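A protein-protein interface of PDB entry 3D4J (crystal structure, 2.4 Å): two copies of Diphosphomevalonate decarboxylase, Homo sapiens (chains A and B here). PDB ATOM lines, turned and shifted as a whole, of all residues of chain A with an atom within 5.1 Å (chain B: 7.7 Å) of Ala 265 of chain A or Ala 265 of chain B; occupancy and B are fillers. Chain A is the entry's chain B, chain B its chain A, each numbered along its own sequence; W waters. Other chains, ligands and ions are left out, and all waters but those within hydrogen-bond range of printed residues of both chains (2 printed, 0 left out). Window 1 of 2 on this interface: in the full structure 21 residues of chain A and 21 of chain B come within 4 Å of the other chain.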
ATOM      1  N   LEU A 224     -17.903 -22.661  19.846  1.00  0.00           N
ATOM      2  CA  LEU A 224     -18.382 -23.050  18.524  1.00  0.00           C
ATOM      3  C   LEU A 224     -18.508 -24.571  18.411  1.00  0.00           C
ATOM      4  O   LEU A 224     -19.386 -25.072  17.710  1.00  0.00           O
ATOM      5  CB  LEU A 224     -17.455 -22.510  17.432  1.00  0.00           C
ATOM      6  CG  LEU A 224     -17.329 -20.988  17.364  1.00  0.00           C
ATOM      7  CD1 LEU A 224     -16.395 -20.652  16.227  1.00  0.00           C
ATOM      8  CD2 LEU A 224     -18.697 -20.322  17.162  1.00  0.00           C
ATOM      9  N   ASN A 261     -13.301 -28.163   7.145  1.00  0.00           N
ATOM     10  CA  ASN A 261     -13.081 -26.773   7.499  1.00  0.00           C
ATOM     11  C   ASN A 261     -13.691 -26.367   8.851  1.00  0.00           C
ATOM     12  O   ASN A 261     -13.098 -25.573   9.586  1.00  0.00           O
ATOM     13  CB  ASN A 261     -13.603 -25.865   6.372  1.00  0.00           C
ATOM     14  CG  ASN A 261     -12.799 -26.013   5.076  1.00  0.00           C
ATOM     15  OD1 ASN A 261     -11.609 -26.352   5.098  1.00  0.00           O
ATOM     16  ND2 ASN A 261     -13.440 -25.742   3.951  1.00  0.00           N
ATOM     17  N   GLN A 262     -14.862 -26.905   9.184  1.00  0.00           N
ATOM     18  CA  GLN A 262     -15.492 -26.570  10.455  1.00  0.00           C
ATOM     19  C   GLN A 262     -14.718 -27.222  11.603  1.00  0.00           C
ATOM     20  O   GLN A 262     -14.589 -26.647  12.687  1.00  0.00           O
ATOM     21  CB  GLN A 262     -16.955 -27.023  10.478  1.00  0.00           C
ATOM     22  CG  GLN A 262     -17.728 -26.443  11.661  1.00  0.00           C
ATOM     23  CD  GLN A 262     -19.213 -26.741  11.599  1.00  0.00           C
ATOM     24  OE1 GLN A 262     -19.682 -27.777  12.090  1.00  0.00           O
ATOM     25  NE2 GLN A 262     -19.962 -25.840  10.974  1.00  0.00           N
ATOM     26  N   PHE A 263     -14.205 -28.421  11.365  1.00  0.00           N
ATOM     27  CA  PHE A 263     -13.426 -29.104  12.386  1.00  0.00           C
ATOM     28  C   PHE A 263     -12.232 -28.213  12.749  1.00  0.00           C
ATOM     29  O   PHE A 263     -12.004 -27.907  13.925  1.00  0.00           O
ATOM     30  CB  PHE A 263     -12.962 -30.477  11.858  1.00  0.00           C
ATOM     31  CG  PHE A 263     -11.703 -31.000  12.508  1.00  0.00           C
ATOM     32  CD1 PHE A 263     -11.545 -30.982  13.889  1.00  0.00           C
ATOM     33  CD2 PHE A 263     -10.661 -31.497  11.727  1.00  0.00           C
ATOM     34  CE1 PHE A 263     -10.364 -31.447  14.481  1.00  0.00           C
ATOM     35  CE2 PHE A 263      -9.482 -31.966  12.310  1.00  0.00           C
ATOM     36  CZ  PHE A 263      -9.332 -31.938  13.687  1.00  0.00           C
ATOM     37  N   HIS A 264     -11.488 -27.777  11.736  1.00  0.00           N
ATOM     38  CA  HIS A 264     -10.328 -26.941  11.974  1.00  0.00           C
ATOM     39  C   HIS A 264     -10.691 -25.561  12.514  1.00  0.00           C
ATOM     40  O   HIS A 264      -9.877 -24.906  13.162  1.00  0.00           O
ATOM     41  CB  HIS A 264      -9.489 -26.872  10.695  1.00  0.00           C
ATOM     42  CG  HIS A 264      -8.835 -28.179  10.367  1.00  0.00           C
ATOM     43  ND1 HIS A 264      -7.665 -28.591  10.960  1.00  0.00           N
ATOM     44  CD2 HIS A 264      -9.277 -29.229   9.637  1.00  0.00           C
ATOM     45  CE1 HIS A 264      -7.413 -29.844  10.617  1.00  0.00           C
ATOM     46  NE2 HIS A 264      -8.376 -30.253   9.821  1.00  0.00           N
ATOM     47  N   ALA A 265     -11.924 -25.136  12.267  1.00  0.00           N
ATOM     48  CA  ALA A 265     -12.397 -23.853  12.773  1.00  0.00           C
ATOM     49  C   ALA A 265     -12.572 -23.955  14.299  1.00  0.00           C
ATOM     50  O   ALA A 265     -12.137 -23.071  15.035  1.00  0.00           O
ATOM     51  CB  ALA A 265     -13.721 -23.480  12.121  1.00  0.00           C
ATOM     52  N   THR A 266     -13.200 -25.032  14.770  1.00  0.00           N
ATOM     53  CA  THR A 266     -13.399 -25.190  16.207  1.00  0.00           C
ATOM     54  C   THR A 266     -12.067 -25.403  16.905  1.00  0.00           C
ATOM     55  O   THR A 266     -11.949 -25.135  18.095  1.00  0.00           O
ATOM     56  CB  THR A 266     -14.361 -26.360  16.561  1.00  0.00           C
ATOM     57  OG1 THR A 266     -13.792 -27.607  16.150  1.00  0.00           O
ATOM     58  CG2 THR A 266     -15.703 -26.176  15.875  1.00  0.00           C
ATOM     59  N   CYS A 267     -11.066 -25.882  16.164  1.00  0.00           N
ATOM     60  CA  CYS A 267      -9.732 -26.079  16.727  1.00  0.00           C
ATOM     61  C   CYS A 267      -9.133 -24.711  16.994  1.00  0.00           C
ATOM     62  O   CYS A 267      -8.453 -24.493  18.002  1.00  0.00           O
ATOM     63  CB  CYS A 267      -8.815 -26.808  15.745  1.00  0.00           C
ATOM     64  SG  CYS A 267      -8.990 -28.571  15.714  1.00  0.00           S
ATOM     65  N   LEU A 268      -9.372 -23.794  16.065  1.00  0.00           N
ATOM     66  CA  LEU A 268      -8.854 -22.441  16.193  1.00  0.00           C
ATOM     67  C   LEU A 268      -9.671 -21.662  17.232  1.00  0.00           C
ATOM     68  O   LEU A 268      -9.168 -20.720  17.838  1.00  0.00           O
ATOM     69  CB  LEU A 268      -8.866 -21.763  14.811  1.00  0.00           C
ATOM     70  CG  LEU A 268      -8.535 -20.291  14.524  1.00  0.00           C
ATOM     71  CD1 LEU A 268      -7.420 -19.726  15.438  1.00  0.00           C
ATOM     72  CD2 LEU A 268      -8.135 -20.204  13.039  1.00  0.00           C
ATOM     73  N   ASP A 269     -10.919 -22.080  17.446  1.00  0.00           N
ATOM     74  CA  ASP A 269     -11.799 -21.435  18.428  1.00  0.00           C
ATOM     75  C   ASP A 269     -11.450 -21.969  19.824  1.00  0.00           C
ATOM     76  O   ASP A 269     -12.069 -21.591  20.821  1.00  0.00           O
ATOM     77  CB  ASP A 269     -13.277 -21.739  18.114  1.00  0.00           C
ATOM     78  CG  ASP A 269     -14.251 -21.092  19.115  1.00  0.00           C
ATOM     79  OD1 ASP A 269     -14.383 -19.848  19.129  1.00  0.00           O
ATOM     80  OD2 ASP A 269     -14.892 -21.834  19.894  1.00  0.00           O
ATOM     81  N   SER B 222     -21.119 -19.495   6.401  1.00  0.00           N
ATOM     82  CA  SER B 222     -20.628 -19.988   7.691  1.00  0.00           C
ATOM     83  C   SER B 222     -21.670 -20.187   8.775  1.00  0.00           C
ATOM     84  O   SER B 222     -22.073 -19.240   9.455  1.00  0.00           O
ATOM     85  CB  SER B 222     -19.527 -19.067   8.229  1.00  0.00           C
ATOM     86  OG  SER B 222     -19.032 -19.542   9.470  1.00  0.00           O
ATOM     87  N   LEU B 224     -21.251 -21.298  11.561  1.00  0.00           N
ATOM     88  CA  LEU B 224     -20.683 -20.919  12.856  1.00  0.00           C
ATOM     89  C   LEU B 224     -20.728 -19.402  13.053  1.00  0.00           C
ATOM     90  O   LEU B 224     -20.828 -18.919  14.180  1.00  0.00           O
ATOM     91  CB  LEU B 224     -19.241 -21.416  12.985  1.00  0.00           C
ATOM     92  CG  LEU B 224     -19.031 -22.936  13.007  1.00  0.00           C
ATOM     93  CD1 LEU B 224     -17.563 -23.223  13.272  1.00  0.00           C
ATOM     94  CD2 LEU B 224     -19.895 -23.586  14.097  1.00  0.00           C
ATOM     95  N   LEU B 225     -20.655 -18.654  11.955  1.00  0.00           N
ATOM     96  CA  LEU B 225     -20.694 -17.198  12.031  1.00  0.00           C
ATOM     97  C   LEU B 225     -22.046 -16.723  12.545  1.00  0.00           C
ATOM     98  O   LEU B 225     -22.131 -15.721  13.255  1.00  0.00           O
ATOM     99  CB  LEU B 225     -20.430 -16.564  10.656  1.00  0.00           C
ATOM    100  CG  LEU B 225     -20.517 -15.030  10.642  1.00  0.00           C
ATOM    101  CD1 LEU B 225     -19.544 -14.471  11.667  1.00  0.00           C
ATOM    102  CD2 LEU B 225     -20.209 -14.471   9.265  1.00  0.00           C
ATOM    103  N   ARG B 228     -22.095 -17.211  16.260  1.00  0.00           N
ATOM    104  CA  ARG B 228     -21.213 -16.249  16.897  1.00  0.00           C
ATOM    105  C   ARG B 228     -21.968 -14.945  17.177  1.00  0.00           C
ATOM    106  O   ARG B 228     -21.926 -14.431  18.289  1.00  0.00           O
ATOM    107  CB  ARG B 228     -19.996 -15.970  16.005  1.00  0.00           C
ATOM    108  CG  ARG B 228     -19.210 -14.719  16.382  1.00  0.00           C
ATOM    109  CD  ARG B 228     -18.133 -14.358  15.353  1.00  0.00           C
ATOM    110  NE  ARG B 228     -17.606 -13.010  15.571  1.00  0.00           N
ATOM    111  CZ  ARG B 228     -16.885 -12.648  16.629  1.00  0.00           C
ATOM    112  NH1 ARG B 228     -16.591 -13.536  17.573  1.00  0.00           N
ATOM    113  NH2 ARG B 228     -16.480 -11.391  16.754  1.00  0.00           N
ATOM    114  N   LYS B 258      -9.497 -14.793  22.535  1.00  0.00           N
ATOM    115  CA  LYS B 258     -10.564 -15.714  22.167  1.00  0.00           C
ATOM    116  C   LYS B 258     -11.435 -15.154  21.041  1.00  0.00           C
ATOM    117  O   LYS B 258     -11.938 -15.901  20.204  1.00  0.00           O
ATOM    118  CB  LYS B 258     -11.447 -16.043  23.378  1.00  0.00           C
ATOM    119  CG  LYS B 258     -10.729 -16.745  24.522  1.00  0.00           C
ATOM    120  CD  LYS B 258     -11.645 -16.874  25.731  1.00  0.00           C
ATOM    121  CE  LYS B 258     -10.933 -17.529  26.908  1.00  0.00           C
ATOM    122  NZ  LYS B 258     -11.807 -17.580  28.128  1.00  0.00           N
ATOM    123  N   ASP B 259     -11.606 -13.838  21.010  1.00  0.00           N
ATOM    124  CA  ASP B 259     -12.439 -13.259  19.977  1.00  0.00           C
ATOM    125  C   ASP B 259     -11.679 -13.111  18.662  1.00  0.00           C
ATOM    126  O   ASP B 259     -12.283 -13.145  17.591  1.00  0.00           O
ATOM    127  CB  ASP B 259     -13.025 -11.915  20.419  1.00  0.00           C
ATOM    128  CG  ASP B 259     -14.362 -11.647  19.771  1.00  0.00           C
ATOM    129  OD1 ASP B 259     -14.461 -10.719  18.951  1.00  0.00           O
ATOM    130  OD2 ASP B 259     -15.316 -12.392  20.074  1.00  0.00           O
ATOM    131  N   SER B 260     -10.364 -12.937  18.741  1.00  0.00           N
ATOM    132  CA  SER B 260      -9.570 -12.860  17.524  1.00  0.00           C
ATOM    133  C   SER B 260      -9.620 -14.252  16.920  1.00  0.00           C
ATOM    134  O   SER B 260      -9.868 -14.416  15.724  1.00  0.00           O
ATOM    135  CB  SER B 260      -8.108 -12.522  17.822  1.00  0.00           C
ATOM    136  OG  SER B 260      -7.319 -12.595  16.640  1.00  0.00           O
ATOM    137  N   ASN B 261      -9.410 -15.253  17.770  1.00  0.00           N
ATOM    138  CA  ASN B 261      -9.387 -16.630  17.310  1.00  0.00           C
ATOM    139  C   ASN B 261     -10.697 -17.082  16.710  1.00  0.00           C
ATOM    140  O   ASN B 261     -10.702 -17.821  15.727  1.00  0.00           O
ATOM    141  CB  ASN B 261      -8.976 -17.580  18.437  1.00  0.00           C
ATOM    142  CG  ASN B 261      -7.538 -17.368  18.875  1.00  0.00           C
ATOM    143  OD1 ASN B 261      -6.706 -16.924  18.093  1.00  0.00           O
ATOM    144  ND2 ASN B 261      -7.241 -17.695  20.127  1.00  0.00           N
ATOM    145  N   GLN B 262     -11.805 -16.622  17.280  1.00  0.00           N
ATOM    146  CA  GLN B 262     -13.106 -17.014  16.772  1.00  0.00           C
ATOM    147  C   GLN B 262     -13.379 -16.368  15.414  1.00  0.00           C
ATOM    148  O   GLN B 262     -13.991 -16.982  14.541  1.00  0.00           O
ATOM    149  CB  GLN B 262     -14.203 -16.634  17.770  1.00  0.00           C
ATOM    150  CG  GLN B 262     -15.534 -17.330  17.510  1.00  0.00           C
ATOM    151  CD  GLN B 262     -16.532 -17.103  18.643  1.00  0.00           C
ATOM    152  OE1 GLN B 262     -17.258 -16.099  18.671  1.00  0.00           O
ATOM    153  NE2 GLN B 262     -16.555 -18.032  19.595  1.00  0.00           N
ATOM    154  N   PHE B 263     -12.936 -15.126  15.245  1.00  0.00           N
ATOM    155  CA  PHE B 263     -13.132 -14.425  13.979  1.00  0.00           C
ATOM    156  C   PHE B 263     -12.471 -15.265  12.886  1.00  0.00           C
ATOM    157  O   PHE B 263     -13.135 -15.687  11.942  1.00  0.00           O
ATOM    158  CB  PHE B 263     -12.534 -13.001  14.056  1.00  0.00           C
ATOM    159  CG  PHE B 263     -12.068 -12.450  12.727  1.00  0.00           C
ATOM    160  CD1 PHE B 263     -12.867 -12.546  11.582  1.00  0.00           C
ATOM    161  CD2 PHE B 263     -10.795 -11.876  12.609  1.00  0.00           C
ATOM    162  CE1 PHE B 263     -12.398 -12.088  10.341  1.00  0.00           C
ATOM    163  CE2 PHE B 263     -10.323 -11.413  11.372  1.00  0.00           C
ATOM    164  CZ  PHE B 263     -11.126 -11.522  10.232  1.00  0.00           C
ATOM    165  N   HIS B 264     -11.176 -15.532  13.033  1.00  0.00           N
ATOM    166  CA  HIS B 264     -10.448 -16.348  12.054  1.00  0.00           C
ATOM    167  C   HIS B 264     -11.054 -17.741  11.940  1.00  0.00           C
ATOM    168  O   HIS B 264     -10.975 -18.383  10.887  1.00  0.00           O
ATOM    169  CB  HIS B 264      -8.965 -16.422  12.425  1.00  0.00           C
ATOM    170  CG  HIS B 264      -8.246 -15.132  12.209  1.00  0.00           C
ATOM    171  ND1 HIS B 264      -7.873 -14.693  10.955  1.00  0.00           N
ATOM    172  CD2 HIS B 264      -7.959 -14.118  13.061  1.00  0.00           C
ATOM    173  CE1 HIS B 264      -7.397 -13.466  11.041  1.00  0.00           C
ATOM    174  NE2 HIS B 264      -7.442 -13.092  12.310  1.00  0.00           N
ATOM    175  N   ALA B 265     -11.671 -18.198  13.021  1.00  0.00           N
ATOM    176  CA  ALA B 265     -12.322 -19.502  13.013  1.00  0.00           C
ATOM    177  C   ALA B 265     -13.472 -19.465  12.011  1.00  0.00           C
ATOM    178  O   ALA B 265     -13.641 -20.393  11.217  1.00  0.00           O
ATOM    179  CB  ALA B 265     -12.861 -19.833  14.386  1.00  0.00           C
ATOM    180  N   THR B 266     -14.257 -18.389  12.045  1.00  0.00           N
ATOM    181  CA  THR B 266     -15.387 -18.271  11.134  1.00  0.00           C
ATOM    182  C   THR B 266     -14.897 -18.111   9.694  1.00  0.00           C
ATOM    183  O   THR B 266     -15.607 -18.471   8.752  1.00  0.00           O
ATOM    184  CB  THR B 266     -16.339 -17.087  11.509  1.00  0.00           C
ATOM    185  OG1 THR B 266     -15.634 -15.851  11.439  1.00  0.00           O
ATOM    186  CG2 THR B 266     -16.888 -17.251  12.921  1.00  0.00           C
ATOM    187  N   CYS B 267     -13.693 -17.576   9.512  1.00  0.00           N
ATOM    188  CA  CYS B 267     -13.163 -17.432   8.150  1.00  0.00           C
ATOM    189  C   CYS B 267     -12.835 -18.814   7.598  1.00  0.00           C
ATOM    190  O   CYS B 267     -12.987 -19.075   6.401  1.00  0.00           O
ATOM    191  CB  CYS B 267     -11.903 -16.574   8.132  1.00  0.00           C
ATOM    192  SG  CYS B 267     -12.222 -14.832   8.463  1.00  0.00           S
ATOM    193  N   LEU B 268     -12.400 -19.696   8.490  1.00  0.00           N
ATOM    194  CA  LEU B 268     -12.051 -21.055   8.120  1.00  0.00           C
ATOM    195  C   LEU B 268     -13.318 -21.851   7.846  1.00  0.00           C
ATOM    196  O   LEU B 268     -13.299 -22.790   7.055  1.00  0.00           O
ATOM    197  CB  LEU B 268     -11.231 -21.685   9.246  1.00  0.00           C
ATOM    198  CG  LEU B 268     -10.450 -22.994   9.113  1.00  0.00           C
ATOM    199  CD1 LEU B 268     -10.193 -23.360   7.640  1.00  0.00           C
ATOM    200  CD2 LEU B 268      -9.141 -22.846   9.901  1.00  0.00           C
ATOM    201  N   ASP B 269     -14.420 -21.456   8.490  1.00  0.00           N
ATOM    202  CA  ASP B 269     -15.724 -22.109   8.327  1.00  0.00           C
ATOM    203  C   ASP B 269     -16.482 -21.558   7.113  1.00  0.00           C
ATOM    204  O   ASP B 269     -17.575 -21.992   6.790  1.00  0.00           O
ATOM    205  CB  ASP B 269     -16.565 -21.903   9.591  1.00  0.00           C
ATOM    206  CG  ASP B 269     -17.876 -22.672   9.560  1.00  0.00           C
ATOM    207  OD1 ASP B 269     -17.836 -23.914   9.433  1.00  0.00           O
ATOM    208  OD2 ASP B 269     -18.948 -22.031   9.669  1.00  0.00           O
ATOM    209  N   THR B 270     -15.905 -20.573   6.453  1.00  0.00           N
ATOM    210  CA  THR B 270     -16.522 -20.001   5.274  1.00  0.00           C
ATOM    211  C   THR B 270     -16.195 -20.984   4.128  1.00  0.00           C
ATOM    212  O   THR B 270     -15.261 -21.786   4.245  1.00  0.00           O
ATOM    213  CB  THR B 270     -15.938 -18.583   5.010  1.00  0.00           C
ATOM    214  OG1 THR B 270     -16.172 -17.764   6.159  1.00  0.00           O
ATOM    215  CG2 THR B 270     -16.582 -17.916   3.797  1.00  0.00           C
ATOM    216  N   ILE B 274     -11.395 -19.110   4.204  1.00  0.00           N
ATOM    217  CA  ILE B 274     -10.542 -17.935   4.082  1.00  0.00           C
ATOM    218  C   ILE B 274      -9.385 -18.097   5.052  1.00  0.00           C
ATOM    219  O   ILE B 274      -9.554 -18.652   6.145  1.00  0.00           O
ATOM    220  CB  ILE B 274     -11.318 -16.637   4.379  1.00  0.00           C
ATOM    221  CG1 ILE B 274     -12.487 -16.490   3.394  1.00  0.00           C
ATOM    222  CG2 ILE B 274     -10.394 -15.436   4.250  1.00  0.00           C
ATOM    223  CD1 ILE B 274     -13.346 -15.241   3.639  1.00  0.00           C
ATOM    224  N   LEU B 277      -4.198 -15.821   8.705  1.00  0.00           N
ATOM    225  CA  LEU B 277      -3.044 -16.089   9.546  1.00  0.00           C
ATOM    226  C   LEU B 277      -1.994 -16.908   8.798  1.00  0.00           C
ATOM    227  O   LEU B 277      -2.333 -17.907   8.169  1.00  0.00           O
ATOM    228  CB  LEU B 277      -3.465 -16.879  10.791  1.00  0.00           C
ATOM    229  CG  LEU B 277      -4.544 -16.281  11.697  1.00  0.00           C
ATOM    230  CD1 LEU B 277      -4.661 -17.139  12.968  1.00  0.00           C
ATOM    231  CD2 LEU B 277      -4.191 -14.835  12.056  1.00  0.00           C
HETATM  232  O   HOH W   1     -13.360 -18.165  20.760  1.00  0.00           O
HETATM  233  O   HOH W   2     -15.927 -24.263   4.541  1.00  0.00           O
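The side-chain carboxylate of Asp 269 of chain B lies within hydrogen-bond range of the side-chain hydroxyl of Ser 222 of chain B, 2.5 Å away.
The backbone NH (N) of Leu 224 of chain B lies within hydrogen-bond range of the side-chain carboxylate (OD2) of Asp 269 of chain B, at 3.1 Å.
NH1 of Arg 228 of chain B lies within hydrogen-bond range of OE1 of Gln 262 of chain B (2.9 Å).
The backbone NH of Leu 224 of chain A lies within hydrogen-bond range of the side-chain carboxylate of Asp 269 of chain A.
Of the 19 printed residues of chain B, 7 touch a printed residue of chain A.
Along chain B the printed residues that touch a printed residue of chain A span positions 224 to 269.
Among the printed residues, no Asp or Glu carboxylate lies within 4 Å of a Lys or Arg side-chain nitrogen of the other chain.
CD2 of Leu 224 of chain A touches O of Leu 224 of chain B (3.9 Å).
Leu 224 of chain A touches Gln 262 of chain B.
Leu 268 of chain B touches Asn 261 of chain A.
CD1 of Leu 224 of chain B touches CG of Gln 262 of chain A, 3.6 Å away.
CD2 of Leu 268 of chain B touches O of His 264 of chain A, at 3.9 Å.
Ala 265 of chain A touches Ala 265 of chain B.
O of Leu 268 of chain A touches CB of Asn 261 of chain B, at 3.2 Å.
Leu 268 of chain A touches His 264 of chain B (CD2 to CB, 3.9 Å).
Water W1 lies within hydrogen-bond range of OD1 of Asp 269 of chain A, O of Lys 258 of chain B and NE2 of Gln 262 of chain B.
Water W2 lies within hydrogen-bond range of O of Thr 270 of chain B (2.6 Å) and ND2 of Asn 261 of chain A (3.0 Å).
NE2 of Gln 262 of chain B is in hydrogen-bond range of OD1 of Asp 269 of chain A, at 2.9 Å.
The side-chain carboxylate of Asp 269 of chain B sits at hydrogen-bond distance from the side-chain amide nitrogen of Gln 262 of chain A, 3.3 Å away.
Printed residues of chain B within 4 Å of Ala 265 of chain A: Ala 265.
Ala 265 of chain B touches just one residue of chain A: Ala 265 (3.2 Å).
Of the printed residues of chain A, Asn 261 of chain B touches Leu 268.
Printed residues of chain B within 4 Å of Gln 262 of chain A: Leu 224 (3.6 Å) and Asp 269 (3.3 Å).
Cys 267 of chain B touches none of the printed residues of chain A.
Ile 274 of chain B touches none of the printed residues of chain A.
The nearest printed residue of chain B that does not touch Ala 265 of chain A is Leu 224 of chain B (4.02 Å).
Leu 224 of chain A touches its own counterpart, Leu 224 of chain B.
Asn 261 of chain A touches Leu 268 of chain B, and with the chains exchanged Leu 268 of chain A touches Asn 261 of chain B.
Gln 262 of chain A touches Asp 269 of chain B, and with the chains exchanged Asp 269 of chain A touches Gln 262 of chain B.
Ala 265 of chain A touches its own counterpart, Ala 265 of chain B.
Positions printed for both chains: 224, 261, 262, 263, 264, 265, 266, 267, 268 and 269.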
